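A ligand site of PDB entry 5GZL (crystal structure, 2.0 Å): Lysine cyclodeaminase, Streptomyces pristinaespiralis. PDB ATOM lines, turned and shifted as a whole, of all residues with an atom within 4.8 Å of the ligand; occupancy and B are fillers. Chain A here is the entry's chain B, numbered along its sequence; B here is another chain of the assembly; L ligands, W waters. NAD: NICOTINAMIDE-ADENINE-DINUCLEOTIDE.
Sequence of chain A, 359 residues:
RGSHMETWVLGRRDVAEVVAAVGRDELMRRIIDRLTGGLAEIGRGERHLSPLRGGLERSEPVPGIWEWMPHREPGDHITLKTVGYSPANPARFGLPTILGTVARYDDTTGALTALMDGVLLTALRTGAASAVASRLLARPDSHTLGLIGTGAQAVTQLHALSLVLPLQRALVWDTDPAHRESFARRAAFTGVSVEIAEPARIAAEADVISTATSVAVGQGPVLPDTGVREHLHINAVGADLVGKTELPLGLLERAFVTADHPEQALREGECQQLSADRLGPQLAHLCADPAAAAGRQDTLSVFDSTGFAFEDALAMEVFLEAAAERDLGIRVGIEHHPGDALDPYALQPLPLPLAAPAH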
ATOM      1  N   TYR A  85      17.447 -13.535 -17.810  1.00  0.00           N
ATOM      2  CA  TYR A  85      16.537 -12.970 -16.807  1.00  0.00           C
ATOM      3  C   TYR A  85      17.190 -11.619 -16.428  1.00  0.00           C
ATOM      4  O   TYR A  85      18.307 -11.603 -15.941  1.00  0.00           O
ATOM      5  CB  TYR A  85      16.497 -13.876 -15.634  1.00  0.00           C
ATOM      6  CG  TYR A  85      15.991 -13.247 -14.348  1.00  0.00           C
ATOM      7  CD1 TYR A  85      14.630 -13.017 -14.144  1.00  0.00           C
ATOM      8  CD2 TYR A  85      16.864 -12.914 -13.327  1.00  0.00           C
ATOM      9  CE1 TYR A  85      14.148 -12.460 -12.972  1.00  0.00           C
ATOM     10  CE2 TYR A  85      16.410 -12.350 -12.138  1.00  0.00           C
ATOM     11  CZ  TYR A  85      15.043 -12.144 -11.963  1.00  0.00           C
ATOM     12  OH  TYR A  85      14.562 -11.610 -10.782  1.00  0.00           O
ATOM     13  N   PRO A  90      11.630  -4.415 -18.113  1.00  0.00           N
ATOM     14  CA  PRO A  90      10.342  -3.793 -18.414  1.00  0.00           C
ATOM     15  C   PRO A  90      10.342  -2.273 -18.214  1.00  0.00           C
ATOM     16  O   PRO A  90       9.973  -1.550 -19.132  1.00  0.00           O
ATOM     17  CB  PRO A  90       9.391  -4.445 -17.385  1.00  0.00           C
ATOM     18  CG  PRO A  90      10.002  -5.801 -17.142  1.00  0.00           C
ATOM     19  CD  PRO A  90      11.480  -5.527 -17.162  1.00  0.00           C
ATOM     20  N   THR A  97      11.452  -9.017 -18.927  1.00  0.00           N
ATOM     21  CA  THR A  97      12.476  -9.603 -18.050  1.00  0.00           C
ATOM     22  C   THR A  97      13.084 -10.904 -18.611  1.00  0.00           C
ATOM     23  O   THR A  97      14.320 -11.073 -18.631  1.00  0.00           O
ATOM     24  CB  THR A  97      11.826  -9.879 -16.679  1.00  0.00           C
ATOM     25  OG1 THR A  97      11.495  -8.619 -16.046  1.00  0.00           O
ATOM     26  CG2 THR A  97      12.749 -10.643 -15.768  1.00  0.00           C
ATOM     27  N   ILE A  98      12.213 -11.787 -19.110  1.00  0.00           N
ATOM     28  CA  ILE A  98      12.644 -13.071 -19.720  1.00  0.00           C
ATOM     29  C   ILE A  98      12.691 -12.924 -21.230  1.00  0.00           C
ATOM     30  O   ILE A  98      11.695 -12.653 -21.847  1.00  0.00           O
ATOM     31  CB  ILE A  98      11.691 -14.228 -19.334  1.00  0.00           C
ATOM     32  CG1 ILE A  98      11.754 -14.503 -17.834  1.00  0.00           C
ATOM     33  CG2 ILE A  98      11.962 -15.524 -20.116  1.00  0.00           C
ATOM     34  CD1 ILE A  98      13.113 -14.976 -17.385  1.00  0.00           C
ATOM     35  N   THR A 122       8.349 -19.754 -23.694  1.00  0.00           N
ATOM     36  CA  THR A 122       8.707 -19.917 -22.265  1.00  0.00           C
ATOM     37  C   THR A 122       7.442 -19.707 -21.416  1.00  0.00           C
ATOM     38  O   THR A 122       7.127 -20.511 -20.517  1.00  0.00           O
ATOM     39  CB  THR A 122       9.874 -18.998 -21.827  1.00  0.00           C
ATOM     40  OG1 THR A 122      11.064 -19.386 -22.482  1.00  0.00           O
ATOM     41  CG2 THR A 122      10.151 -19.089 -20.329  1.00  0.00           C
ATOM     42  N   ARG A 125       4.931 -22.753 -21.768  1.00  0.00           N
ATOM     43  CA  ARG A 125       5.265 -24.025 -21.169  1.00  0.00           C
ATOM     44  C   ARG A 125       5.409 -23.948 -19.658  1.00  0.00           C
ATOM     45  O   ARG A 125       5.260 -24.955 -18.986  1.00  0.00           O
ATOM     46  CB  ARG A 125       6.478 -24.733 -21.820  1.00  0.00           C
ATOM     47  CG  ARG A 125       7.853 -24.150 -21.768  1.00  0.00           C
ATOM     48  CD  ARG A 125       8.420 -23.944 -20.380  1.00  0.00           C
ATOM     49  NE  ARG A 125       9.871 -23.939 -20.404  1.00  0.00           N
ATOM     50  CZ  ARG A 125      10.637 -23.607 -19.391  1.00  0.00           C
ATOM     51  NH1 ARG A 125      10.082 -23.147 -18.296  1.00  0.00           N
ATOM     52  NH2 ARG A 125      11.973 -23.753 -19.448  1.00  0.00           N
ATOM     53  N   THR A 126       5.633 -22.752 -19.139  1.00  0.00           N
ATOM     54  CA  THR A 126       5.780 -22.506 -17.722  1.00  0.00           C
ATOM     55  C   THR A 126       4.425 -22.476 -17.067  1.00  0.00           C
ATOM     56  O   THR A 126       4.237 -23.075 -16.062  1.00  0.00           O
ATOM     57  CB  THR A 126       6.537 -21.243 -17.468  1.00  0.00           C
ATOM     58  OG1 THR A 126       7.829 -21.320 -18.070  1.00  0.00           O
ATOM     59  CG2 THR A 126       6.689 -20.981 -15.951  1.00  0.00           C
ATOM     60  N   ILE A 148       1.264 -14.286  -6.580  1.00  0.00           N
ATOM     61  CA  ILE A 148       2.183 -13.359  -6.046  1.00  0.00           C
ATOM     62  C   ILE A 148       3.182 -13.081  -7.136  1.00  0.00           C
ATOM     63  O   ILE A 148       3.917 -13.985  -7.578  1.00  0.00           O
ATOM     64  CB  ILE A 148       2.906 -13.832  -4.768  1.00  0.00           C
ATOM     65  CG1 ILE A 148       1.916 -14.364  -3.731  1.00  0.00           C
ATOM     66  CG2 ILE A 148       3.798 -12.736  -4.213  1.00  0.00           C
ATOM     67  CD1 ILE A 148       1.000 -13.414  -3.095  1.00  0.00           C
ATOM     68  N   GLY A 149       3.269 -11.808  -7.526  1.00  0.00           N
ATOM     69  CA  GLY A 149       3.962 -11.439  -8.733  1.00  0.00           C
ATOM     70  C   GLY A 149       2.982 -11.421  -9.883  1.00  0.00           C
ATOM     71  O   GLY A 149       2.417 -12.449 -10.221  1.00  0.00           O
ATOM     72  N   THR A 150       2.727 -10.237 -10.453  1.00  0.00           N
ATOM     73  CA  THR A 150       1.758 -10.130 -11.550  1.00  0.00           C
ATOM     74  C   THR A 150       2.439  -9.564 -12.801  1.00  0.00           C
ATOM     75  O   THR A 150       1.919  -8.693 -13.433  1.00  0.00           O
ATOM     76  CB  THR A 150       0.544  -9.276 -11.183  1.00  0.00           C
ATOM     77  OG1 THR A 150       0.957  -7.949 -10.783  1.00  0.00           O
ATOM     78  CG2 THR A 150      -0.274  -9.921 -10.086  1.00  0.00           C
ATOM     79  N   GLY A 151       3.620 -10.064 -13.142  1.00  0.00           N
ATOM     80  CA  GLY A 151       4.272  -9.691 -14.406  1.00  0.00           C
ATOM     81  C   GLY A 151       3.908 -10.667 -15.511  1.00  0.00           C
ATOM     82  O   GLY A 151       2.772 -11.160 -15.597  1.00  0.00           O
ATOM     83  N   ALA A 152       4.901 -11.012 -16.317  1.00  0.00           N
ATOM     84  CA  ALA A 152       4.647 -11.813 -17.522  1.00  0.00           C
ATOM     85  C   ALA A 152       4.198 -13.249 -17.191  1.00  0.00           C
ATOM     86  O   ALA A 152       3.210 -13.732 -17.770  1.00  0.00           O
ATOM     87  CB  ALA A 152       5.858 -11.844 -18.434  1.00  0.00           C
ATOM     88  N   GLN A 153       4.906 -13.944 -16.293  1.00  0.00           N
ATOM     89  CA  GLN A 153       4.535 -15.341 -16.060  1.00  0.00           C
ATOM     90  C   GLN A 153       3.157 -15.461 -15.429  1.00  0.00           C
ATOM     91  O   GLN A 153       2.448 -16.437 -15.667  1.00  0.00           O
ATOM     92  CB  GLN A 153       5.540 -16.042 -15.103  1.00  0.00           C
ATOM     93  CG  GLN A 153       6.946 -16.151 -15.684  1.00  0.00           C
ATOM     94  CD  GLN A 153       6.975 -16.578 -17.176  1.00  0.00           C
ATOM     95  OE1 GLN A 153       6.404 -17.607 -17.551  1.00  0.00           O
ATOM     96  NE2 GLN A 153       7.685 -15.790 -18.003  1.00  0.00           N
ATOM     97  N   ALA A 154       2.774 -14.488 -14.609  1.00  0.00           N
ATOM     98  CA  ALA A 154       1.450 -14.522 -13.984  1.00  0.00           C
ATOM     99  C   ALA A 154       0.346 -14.707 -14.969  1.00  0.00           C
ATOM    100  O   ALA A 154      -0.643 -15.371 -14.696  1.00  0.00           O
ATOM    101  CB  ALA A 154       1.164 -13.259 -13.153  1.00  0.00           C
ATOM    102  N   TRP A 173      -1.224 -10.045  -6.047  1.00  0.00           N
ATOM    103  CA  TRP A 173      -0.366  -9.033  -5.448  1.00  0.00           C
ATOM    104  C   TRP A 173       0.979  -8.908  -6.188  1.00  0.00           C
ATOM    105  O   TRP A 173       1.519  -9.863  -6.733  1.00  0.00           O
ATOM    106  CB  TRP A 173      -0.082  -9.344  -3.978  1.00  0.00           C
ATOM    107  CG  TRP A 173       0.660  -8.287  -3.295  1.00  0.00           C
ATOM    108  CD1 TRP A 173       1.964  -8.319  -2.877  1.00  0.00           C
ATOM    109  CD2 TRP A 173       0.141  -6.995  -2.925  1.00  0.00           C
ATOM    110  NE1 TRP A 173       2.285  -7.109  -2.281  1.00  0.00           N
ATOM    111  CE2 TRP A 173       1.177  -6.304  -2.263  1.00  0.00           C
ATOM    112  CE3 TRP A 173      -1.100  -6.387  -3.046  1.00  0.00           C
ATOM    113  CZ2 TRP A 173       1.024  -5.030  -1.778  1.00  0.00           C
ATOM    114  CZ3 TRP A 173      -1.269  -5.084  -2.511  1.00  0.00           C
ATOM    115  CH2 TRP A 173      -0.208  -4.452  -1.899  1.00  0.00           C
ATOM    116  N   ASP A 174       1.451  -7.677  -6.243  1.00  0.00           N
ATOM    117  CA  ASP A 174       2.758  -7.367  -6.745  1.00  0.00           C
ATOM    118  C   ASP A 174       3.276  -6.235  -5.861  1.00  0.00           C
ATOM    119  O   ASP A 174       2.487  -5.427  -5.415  1.00  0.00           O
ATOM    120  CB  ASP A 174       2.688  -6.895  -8.208  1.00  0.00           C
ATOM    121  CG  ASP A 174       4.019  -7.006  -8.914  1.00  0.00           C
ATOM    122  OD1 ASP A 174       4.867  -6.170  -8.675  1.00  0.00           O
ATOM    123  OD2 ASP A 174       4.173  -7.917  -9.720  1.00  0.00           O
ATOM    124  N   THR A 175       4.572  -6.167  -5.629  1.00  0.00           N
ATOM    125  CA  THR A 175       5.126  -5.023  -4.866  1.00  0.00           C
ATOM    126  C   THR A 175       5.170  -3.749  -5.703  1.00  0.00           C
ATOM    127  O   THR A 175       5.313  -2.689  -5.148  1.00  0.00           O
ATOM    128  CB  THR A 175       6.572  -5.329  -4.409  1.00  0.00           C
ATOM    129  OG1 THR A 175       7.271  -5.879  -5.498  1.00  0.00           O
ATOM    130  CG2 THR A 175       6.613  -6.325  -3.280  1.00  0.00           C
ATOM    131  N   ASP A 176       5.009  -3.833  -7.027  1.00  0.00           N
ATOM    132  CA  ASP A 176       4.866  -2.667  -7.871  1.00  0.00           C
ATOM    133  C   ASP A 176       3.396  -2.374  -8.120  1.00  0.00           C
ATOM    134  O   ASP A 176       2.709  -3.170  -8.771  1.00  0.00           O
ATOM    135  CB  ASP A 176       5.671  -2.872  -9.161  1.00  0.00           C
ATOM    136  CG  ASP A 176       5.676  -1.672 -10.076  1.00  0.00           C
ATOM    137  OD1 ASP A 176       4.691  -0.916 -10.090  1.00  0.00           O
ATOM    138  OD2 ASP A 176       6.680  -1.518 -10.810  1.00  0.00           O
ATOM    139  N   HIS A 179       2.100  -2.604 -11.697  1.00  0.00           N
ATOM    140  CA  HIS A 179       2.031  -4.013 -12.175  1.00  0.00           C
ATOM    141  C   HIS A 179       0.823  -4.782 -11.646  1.00  0.00           C
ATOM    142  O   HIS A 179       0.236  -5.571 -12.426  1.00  0.00           O
ATOM    143  CB  HIS A 179       3.336  -4.742 -11.858  1.00  0.00           C
ATOM    144  CG  HIS A 179       4.510  -4.126 -12.558  1.00  0.00           C
ATOM    145  ND1 HIS A 179       5.739  -4.724 -12.639  1.00  0.00           N
ATOM    146  CD2 HIS A 179       4.599  -2.985 -13.313  1.00  0.00           C
ATOM    147  CE1 HIS A 179       6.569  -3.962 -13.348  1.00  0.00           C
ATOM    148  NE2 HIS A 179       5.891  -2.905 -13.765  1.00  0.00           N
ATOM    149  N   ALA A 212       5.455 -16.031  -8.685  1.00  0.00           N
ATOM    150  CA  ALA A 212       6.274 -15.824  -9.925  1.00  0.00           C
ATOM    151  C   ALA A 212       6.803 -14.410  -9.925  1.00  0.00           C
ATOM    152  O   ALA A 212       6.292 -13.533 -10.621  1.00  0.00           O
ATOM    153  CB  ALA A 212       5.446 -16.118 -11.170  1.00  0.00           C
ATOM    154  N   THR A 213       7.824 -14.207  -9.098  1.00  0.00           N
ATOM    155  CA  THR A 213       8.317 -12.873  -8.834  1.00  0.00           C
ATOM    156  C   THR A 213       9.763 -12.729  -9.312  1.00  0.00           C
ATOM    157  O   THR A 213      10.531 -13.723  -9.404  1.00  0.00           O
ATOM    158  CB  THR A 213       8.297 -12.519  -7.338  1.00  0.00           C
ATOM    159  OG1 THR A 213       9.340 -13.201  -6.646  1.00  0.00           O
ATOM    160  CG2 THR A 213       6.951 -12.787  -6.688  1.00  0.00           C
ATOM    161  N   SER A 214      10.145 -11.464  -9.512  1.00  0.00           N
ATOM    162  CA  SER A 214      11.543 -11.097  -9.662  1.00  0.00           C
ATOM    163  C   SER A 214      12.190 -10.698  -8.369  1.00  0.00           C
ATOM    164  O   SER A 214      13.099  -9.887  -8.385  1.00  0.00           O
ATOM    165  CB  SER A 214      11.688 -10.009 -10.685  1.00  0.00           C
ATOM    166  OG  SER A 214      10.892  -8.910 -10.324  1.00  0.00           O
ATOM    167  N   VAL A 215      11.825 -11.342  -7.254  1.00  0.00           N
ATOM    168  CA  VAL A 215      12.432 -11.012  -5.980  1.00  0.00           C
ATOM    169  C   VAL A 215      13.956 -11.291  -6.056  1.00  0.00           C
ATOM    170  O   VAL A 215      14.434 -12.278  -6.646  1.00  0.00           O
ATOM    171  CB  VAL A 215      11.766 -11.792  -4.821  1.00  0.00           C
ATOM    172  CG1 VAL A 215      12.040 -13.299  -4.876  1.00  0.00           C
ATOM    173  CG2 VAL A 215      12.124 -11.241  -3.476  1.00  0.00           C
ATOM    174  N   VAL A 222       7.960 -13.898  -0.144  1.00  0.00           N
ATOM    175  CA  VAL A 222       6.893 -13.174  -0.804  1.00  0.00           C
ATOM    176  C   VAL A 222       5.508 -13.490  -0.253  1.00  0.00           C
ATOM    177  O   VAL A 222       4.575 -12.897  -0.632  1.00  0.00           O
ATOM    178  CB  VAL A 222       6.949 -13.326  -2.319  1.00  0.00           C
ATOM    179  CG1 VAL A 222       8.368 -13.159  -2.850  1.00  0.00           C
ATOM    180  CG2 VAL A 222       6.339 -14.638  -2.761  1.00  0.00           C
ATOM    181  N   VAL A 237       7.280 -20.775  -8.805  1.00  0.00           N
ATOM    182  CA  VAL A 237       7.763 -20.635 -10.153  1.00  0.00           C
ATOM    183  C   VAL A 237       8.947 -19.702 -10.318  1.00  0.00           C
ATOM    184  O   VAL A 237       9.731 -19.890 -11.238  1.00  0.00           O
ATOM    185  CB  VAL A 237       6.625 -20.169 -11.100  1.00  0.00           C
ATOM    186  CG1 VAL A 237       7.086 -19.944 -12.536  1.00  0.00           C
ATOM    187  CG2 VAL A 237       5.479 -21.162 -11.016  1.00  0.00           C
ATOM    188  N   GLY A 238       9.094 -18.700  -9.463  1.00  0.00           N
ATOM    189  CA  GLY A 238      10.250 -17.818  -9.597  1.00  0.00           C
ATOM    190  C   GLY A 238      11.519 -18.649  -9.454  1.00  0.00           C
ATOM    191  O   GLY A 238      11.557 -19.592  -8.684  1.00  0.00           O
ATOM    192  N   ALA A 239      12.498 -18.326 -10.283  1.00  0.00           N
ATOM    193  CA  ALA A 239      13.713 -19.116 -10.422  1.00  0.00           C
ATOM    194  C   ALA A 239      14.645 -18.336 -11.344  1.00  0.00           C
ATOM    195  O   ALA A 239      14.290 -17.972 -12.472  1.00  0.00           O
ATOM    196  CB  ALA A 239      13.412 -20.531 -10.983  1.00  0.00           C
ATOM    197  N   ASP A 240      15.845 -18.064 -10.841  1.00  0.00           N
ATOM    198  CA  ASP A 240      16.848 -17.377 -11.597  1.00  0.00           C
ATOM    199  C   ASP A 240      18.202 -17.556 -11.005  1.00  0.00           C
ATOM    200  O   ASP A 240      18.902 -18.479 -11.416  1.00  0.00           O
ATOM    201  CB  ASP A 240      16.473 -15.907 -11.852  1.00  0.00           C
ATOM    202  CG  ASP A 240      15.895 -15.224 -10.582  1.00  0.00           C
ATOM    203  OD1 ASP A 240      16.685 -14.934  -9.645  1.00  0.00           O
ATOM    204  OD2 ASP A 240      14.697 -14.907 -10.610  1.00  0.00           O
ATOM    205  N   LYS A 244      18.062 -17.514  -4.754  1.00  0.00           N
ATOM    206  CA  LYS A 244      16.742 -16.885  -4.848  1.00  0.00           C
ATOM    207  C   LYS A 244      15.641 -17.855  -4.445  1.00  0.00           C
ATOM    208  O   LYS A 244      15.535 -18.971  -4.978  1.00  0.00           O
ATOM    209  CB  LYS A 244      16.479 -16.356  -6.276  1.00  0.00           C
ATOM    210  CG  LYS A 244      15.102 -15.671  -6.473  1.00  0.00           C
ATOM    211  CD  LYS A 244      14.221 -16.432  -7.438  1.00  0.00           C
ATOM    212  CE  LYS A 244      12.950 -15.678  -7.726  1.00  0.00           C
ATOM    213  NZ  LYS A 244      13.181 -14.369  -8.355  1.00  0.00           N
ATOM    214  N   SER A 305       9.146 -25.336  -9.184  1.00  0.00           N
ATOM    215  CA  SER A 305       9.368 -25.161 -10.620  1.00  0.00           C
ATOM    216  C   SER A 305      10.613 -24.325 -10.926  1.00  0.00           C
ATOM    217  O   SER A 305      10.706 -23.187 -10.519  1.00  0.00           O
ATOM    218  CB  SER A 305       8.144 -24.583 -11.297  1.00  0.00           C
ATOM    219  OG  SER A 305       8.317 -24.457 -12.710  1.00  0.00           O
ATOM    220  N   THR A 306      11.521 -24.891 -11.725  1.00  0.00           N
ATOM    221  CA  THR A 306      12.731 -24.204 -12.216  1.00  0.00           C
ATOM    222  C   THR A 306      12.763 -24.015 -13.731  1.00  0.00           C
ATOM    223  O   THR A 306      13.429 -23.144 -14.207  1.00  0.00           O
ATOM    224  CB  THR A 306      14.013 -24.943 -11.749  1.00  0.00           C
ATOM    225  OG1 THR A 306      13.992 -26.353 -12.132  1.00  0.00           O
ATOM    226  CG2 THR A 306      14.009 -24.889 -10.208  1.00  0.00           C
ATOM    227  N   GLY A 307      12.050 -24.882 -14.430  1.00  0.00           N
ATOM    228  CA  GLY A 307      12.068 -24.959 -15.875  1.00  0.00           C
ATOM    229  C   GLY A 307      13.226 -25.791 -16.339  1.00  0.00           C
ATOM    230  O   GLY A 307      14.332 -25.688 -15.792  1.00  0.00           O
ATOM    231  N   GLU A 311      11.122 -29.257 -21.614  1.00  0.00           N
ATOM    232  CA  GLU A 311       9.808 -28.589 -21.734  1.00  0.00           C
ATOM    233  C   GLU A 311       9.806 -27.682 -22.952  1.00  0.00           C
ATOM    234  O   GLU A 311       8.790 -27.628 -23.654  1.00  0.00           O
ATOM    235  CB  GLU A 311       9.473 -27.756 -20.489  1.00  0.00           C
ATOM    236  CG  GLU A 311       9.401 -28.553 -19.228  1.00  0.00           C
ATOM    237  CD  GLU A 311       9.270 -27.726 -17.932  1.00  0.00           C
ATOM    238  OE1 GLU A 311       9.744 -26.603 -17.855  1.00  0.00           O
ATOM    239  OE2 GLU A 311       8.676 -28.223 -16.941  1.00  0.00           O
ATOM    240  N   LEU B 342       4.872  -6.946 -19.861  1.00  0.00           N
ATOM    241  CA  LEU B 342       4.355  -7.871 -18.842  1.00  0.00           C
ATOM    242  C   LEU B 342       3.222  -8.730 -19.388  1.00  0.00           C
ATOM    243  O   LEU B 342       2.485  -9.308 -18.616  1.00  0.00           O
ATOM    244  CB  LEU B 342       3.837  -7.063 -17.648  1.00  0.00           C
ATOM    245  CG  LEU B 342       4.758  -6.045 -17.025  1.00  0.00           C
ATOM    246  CD1 LEU B 342       4.058  -5.538 -15.773  1.00  0.00           C
ATOM    247  CD2 LEU B 342       6.102  -6.667 -16.681  1.00  0.00           C
HETATM  248  PA  NAD L   1       8.412 -10.044 -14.680  1.00  0.00           P
HETATM  249  O1A NAD L   1       7.464  -9.933 -15.827  1.00  0.00           O
HETATM  250  O2A NAD L   1       9.502  -9.057 -14.392  1.00  0.00           O
HETATM  251  O5B NAD L   1       7.411 -10.126 -13.429  1.00  0.00           O
HETATM  252  C5B NAD L   1       7.933 -10.267 -12.103  1.00  0.00           C
HETATM  253  C4B NAD L   1       7.079  -9.458 -11.116  1.00  0.00           C
HETATM  254  O4B NAD L   1       7.465  -9.778  -9.794  1.00  0.00           O
HETATM  255  C3B NAD L   1       7.226  -7.948 -11.255  1.00  0.00           C
HETATM  256  O3B NAD L   1       5.976  -7.409 -11.628  1.00  0.00           O
HETATM  257  C2B NAD L   1       7.785  -7.501  -9.921  1.00  0.00           C
HETATM  258  O2B NAD L   1       7.400  -6.183  -9.595  1.00  0.00           O
HETATM  259  C1B NAD L   1       7.240  -8.604  -9.014  1.00  0.00           C
HETATM  260  N9A NAD L   1       7.904  -8.755  -7.748  1.00  0.00           N
HETATM  261  C8A NAD L   1       9.224  -8.578  -7.458  1.00  0.00           C
HETATM  262  N7A NAD L   1       9.430  -8.802  -6.134  1.00  0.00           N
HETATM  263  C5A NAD L   1       8.258  -9.156  -5.607  1.00  0.00           C
HETATM  264  C6A NAD L   1       7.759  -9.477  -4.284  1.00  0.00           C
HETATM  265  N6A NAD L   1       8.602  -9.541  -3.249  1.00  0.00           N
HETATM  266  N1A NAD L   1       6.471  -9.743  -4.151  1.00  0.00           N
HETATM  267  C2A NAD L   1       5.593  -9.672  -5.176  1.00  0.00           C
HETATM  268  N3A NAD L   1       5.976  -9.318  -6.404  1.00  0.00           N
HETATM  269  C4A NAD L   1       7.252  -9.043  -6.652  1.00  0.00           C
HETATM  270  O3  NAD L   1       9.151 -11.514 -14.692  1.00  0.00           O
HETATM  271  PN  NAD L   1       8.422 -12.901 -15.103  1.00  0.00           P
HETATM  272  O1N NAD L   1       7.007 -12.912 -14.656  1.00  0.00           O
HETATM  273  O2N NAD L   1       8.701 -13.211 -16.534  1.00  0.00           O
HETATM  274  O5D NAD L   1       9.332 -13.934 -14.269  1.00  0.00           O
HETATM  275  C5D NAD L   1       9.152 -14.072 -12.852  1.00  0.00           C
HETATM  276  C4D NAD L   1      10.005 -15.177 -12.265  1.00  0.00           C
HETATM  277  O4D NAD L   1       9.672 -16.449 -12.906  1.00  0.00           O
HETATM  278  C3D NAD L   1      11.488 -14.966 -12.520  1.00  0.00           C
HETATM  279  O3D NAD L   1      12.209 -15.489 -11.409  1.00  0.00           O
HETATM  280  C2D NAD L   1      11.752 -15.781 -13.761  1.00  0.00           C
HETATM  281  O2D NAD L   1      13.103 -16.105 -14.004  1.00  0.00           O
HETATM  282  C1D NAD L   1      10.906 -16.988 -13.410  1.00  0.00           C
HETATM  283  N1N NAD L   1      10.655 -17.925 -14.489  1.00  0.00           N
HETATM  284  C2N NAD L   1      10.633 -19.217 -14.139  1.00  0.00           C
HETATM  285  C3N NAD L   1      10.366 -20.183 -15.109  1.00  0.00           C
HETATM  286  C7N NAD L   1      10.204 -21.578 -14.656  1.00  0.00           C
HETATM  287  O7N NAD L   1       9.983 -21.893 -13.439  1.00  0.00           O
HETATM  288  N7N NAD L   1      10.069 -22.465 -15.597  1.00  0.00           N
HETATM  289  C4N NAD L   1      10.227 -19.800 -16.479  1.00  0.00           C
HETATM  290  C5N NAD L   1      10.188 -18.411 -16.775  1.00  0.00           C
HETATM  291  C6N NAD L   1      10.435 -17.500 -15.754  1.00  0.00           C
HETATM  292  O   HOH W   1       9.262 -11.732 -18.723  1.00  0.00           O
HETATM  293  O   HOH W   2       8.208 -24.554 -16.002  1.00  0.00           O
HETATM  294  O   HOH W   3      14.772 -17.687 -15.844  1.00  0.00           O
HETATM  295  O   HOH W   4       8.522  -3.438 -10.771  1.00  0.00           O
HETATM  296  O   HOH W   5       8.416  -9.069 -18.262  1.00  0.00           O
HETATM  297  O   HOH W   6       4.892 -12.624 -12.989  1.00  0.00           O
HETATM  298  O   HOH W   7       8.260  -9.793  -0.343  1.00  0.00           O
HETATM  299  O   HOH W   8      11.109  -7.904  -3.483  1.00  0.00           O
HETATM  300  O   HOH W   9       4.799 -10.341  -1.878  1.00  0.00           O
HETATM  301  O   HOH W  10      10.827  -7.360 -12.873  1.00  0.00           O
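An oxygen (O2A) of the ligand lies within hydrogen-bond range of the side-chain hydroxyl (OG1) of Thr 97 (2.6 Å). The side-chain carboxylate of Asp 174 is in hydrogen-bond range of an oxygen (O3B) of the ligand, at 2.7 Å. The side-chain carboxylate (OD2) of Asp 240 is in hydrogen-bond range of an oxygen (O3D) of the ligand, 2.7 Å away. N of Ala 239 sits at hydrogen-bond distance from O3D of the ligand, at 3.1 Å. O of Ala 239 is in hydrogen-bond range of O2D of the ligand, at 2.7 Å. N of Ala 152 sits at hydrogen-bond distance from O1A of the ligand (2.8 Å). N of Gln 153 lies within hydrogen-bond range of O1N of the ligand, 2.9 Å away. The side-chain amide nitrogen (NE2) of Gln 153 sits at hydrogen-bond distance from an oxygen (O2N) of the ligand, 3.1 Å away. ND1 of His 179 sits at hydrogen-bond distance from O3B of the ligand, 2.9 Å away. An oxygen (O7N) of the ligand is in hydrogen-bond range of the side-chain hydroxyl of Ser 305, at 3.1 Å. O3D of the ligand is in hydrogen-bond range of O of Thr 213, at 3.2 Å. The backbone NH (N) of Ser 214 is in hydrogen-bond range of an oxygen (O4B) of the ligand (3.2 Å). The side-chain amino group (NZ) of Lys 244 lies within hydrogen-bond range of an oxygen (O3D) of the ligand, at 3.4 Å.
Water W10 lies within hydrogen-bond range of O2A of the ligand, OG of Ser 214 and OG1 of Thr 97. Water W5 bridges an oxygen (O1A) of the ligand and the backbone NH of Thr 97. Water W2 lies within hydrogen-bond range of a nitrogen (N7N) of the ligand (2.8 Å), the side-chain carboxylate of Glu 311 (3.2 Å), the guanidinium group of Arg 125 (3.3 Å) and the side-chain hydroxyl of Ser 305 (3.3 Å). Water W9 lies within hydrogen-bond range of O of Val 222 (2.9 Å) and N1A of the ligand (2.9 Å). Water W3 lies within hydrogen-bond range of an oxygen (O2D) of the ligand (2.9 Å) and the backbone carbonyl oxygen (O) of Ala 239 (3.4 Å). Water W4 lies within hydrogen-bond range of the side-chain carboxylate of Asp 176 (2.7 Å) and an oxygen (O2B) of the ligand (3.2 Å).
OD2 of Asp 174 sits at hydrogen-bond distance from N of Thr 150 (2.8 Å). The side-chain carboxylate (OD2) of Asp 240 is in salt-bridge range of the side-chain amino group (NZ) of Lys 244. NH1 of Arg 125 lies within salt-bridge range of OE1 of Glu 311, 3.5 Å away. A ring nitrogen (NE2) of His 179 sits at hydrogen-bond distance from the side-chain carboxylate of Asp 176. O of Thr 213 sits at hydrogen-bond distance from NZ of Lys 244. O of Thr 122 lies within hydrogen-bond range of OG1 of Thr 126 (2.7 Å). The side-chain amino group (NZ) of Lys 244 sits at hydrogen-bond distance from the backbone carbonyl oxygen (O) of Val 215 (3.0 Å). O of Ile 148 is in hydrogen-bond range of N of Ala 212.
The guanidinium group of Arg 125 lies close to a nitrogen (N7N) of the ligand (2.8 Å). The backbone carbonyl oxygen (O) of Val 237 sits close to an oxygen (O7N) of the ligand, 3.0 Å away. N of Gly 307 lies close to N7N of the ligand. CD1 of Tyr 85 touches O2D of the ligand, 3.4 Å away. Ile 98 touches the ligand. CG2 of Thr 122 touches C5N of the ligand, at 3.6 Å. Thr 126 touches the ligand (OG1 to C4N, 3.3 Å). CG2 of Ile 148 touches C2A of the ligand, at 3.7 Å. Gly 149 touches the ligand (CA to N3A, 3.7 Å). CA of Gly 151 touches O5B of the ligand, 3.3 Å away. Thr 175 touches the ligand (OG1 to C4A, 3.4 Å). Asp 176 touches the ligand. Ala 212 touches the ligand. Val 215 touches the ligand. Val 222 touches the ligand. Gly 238 touches the ligand (CA to O3D, 3.5 Å). C of Thr 306 touches O7N of the ligand, at 3.5 Å. Leu 342 of chain B touches the ligand. Of the 34 residues printed, 29 come within 4 Å of the ligand. The nearest printed residue that does not touch the ligand is Pro 90 (4.3 Å).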
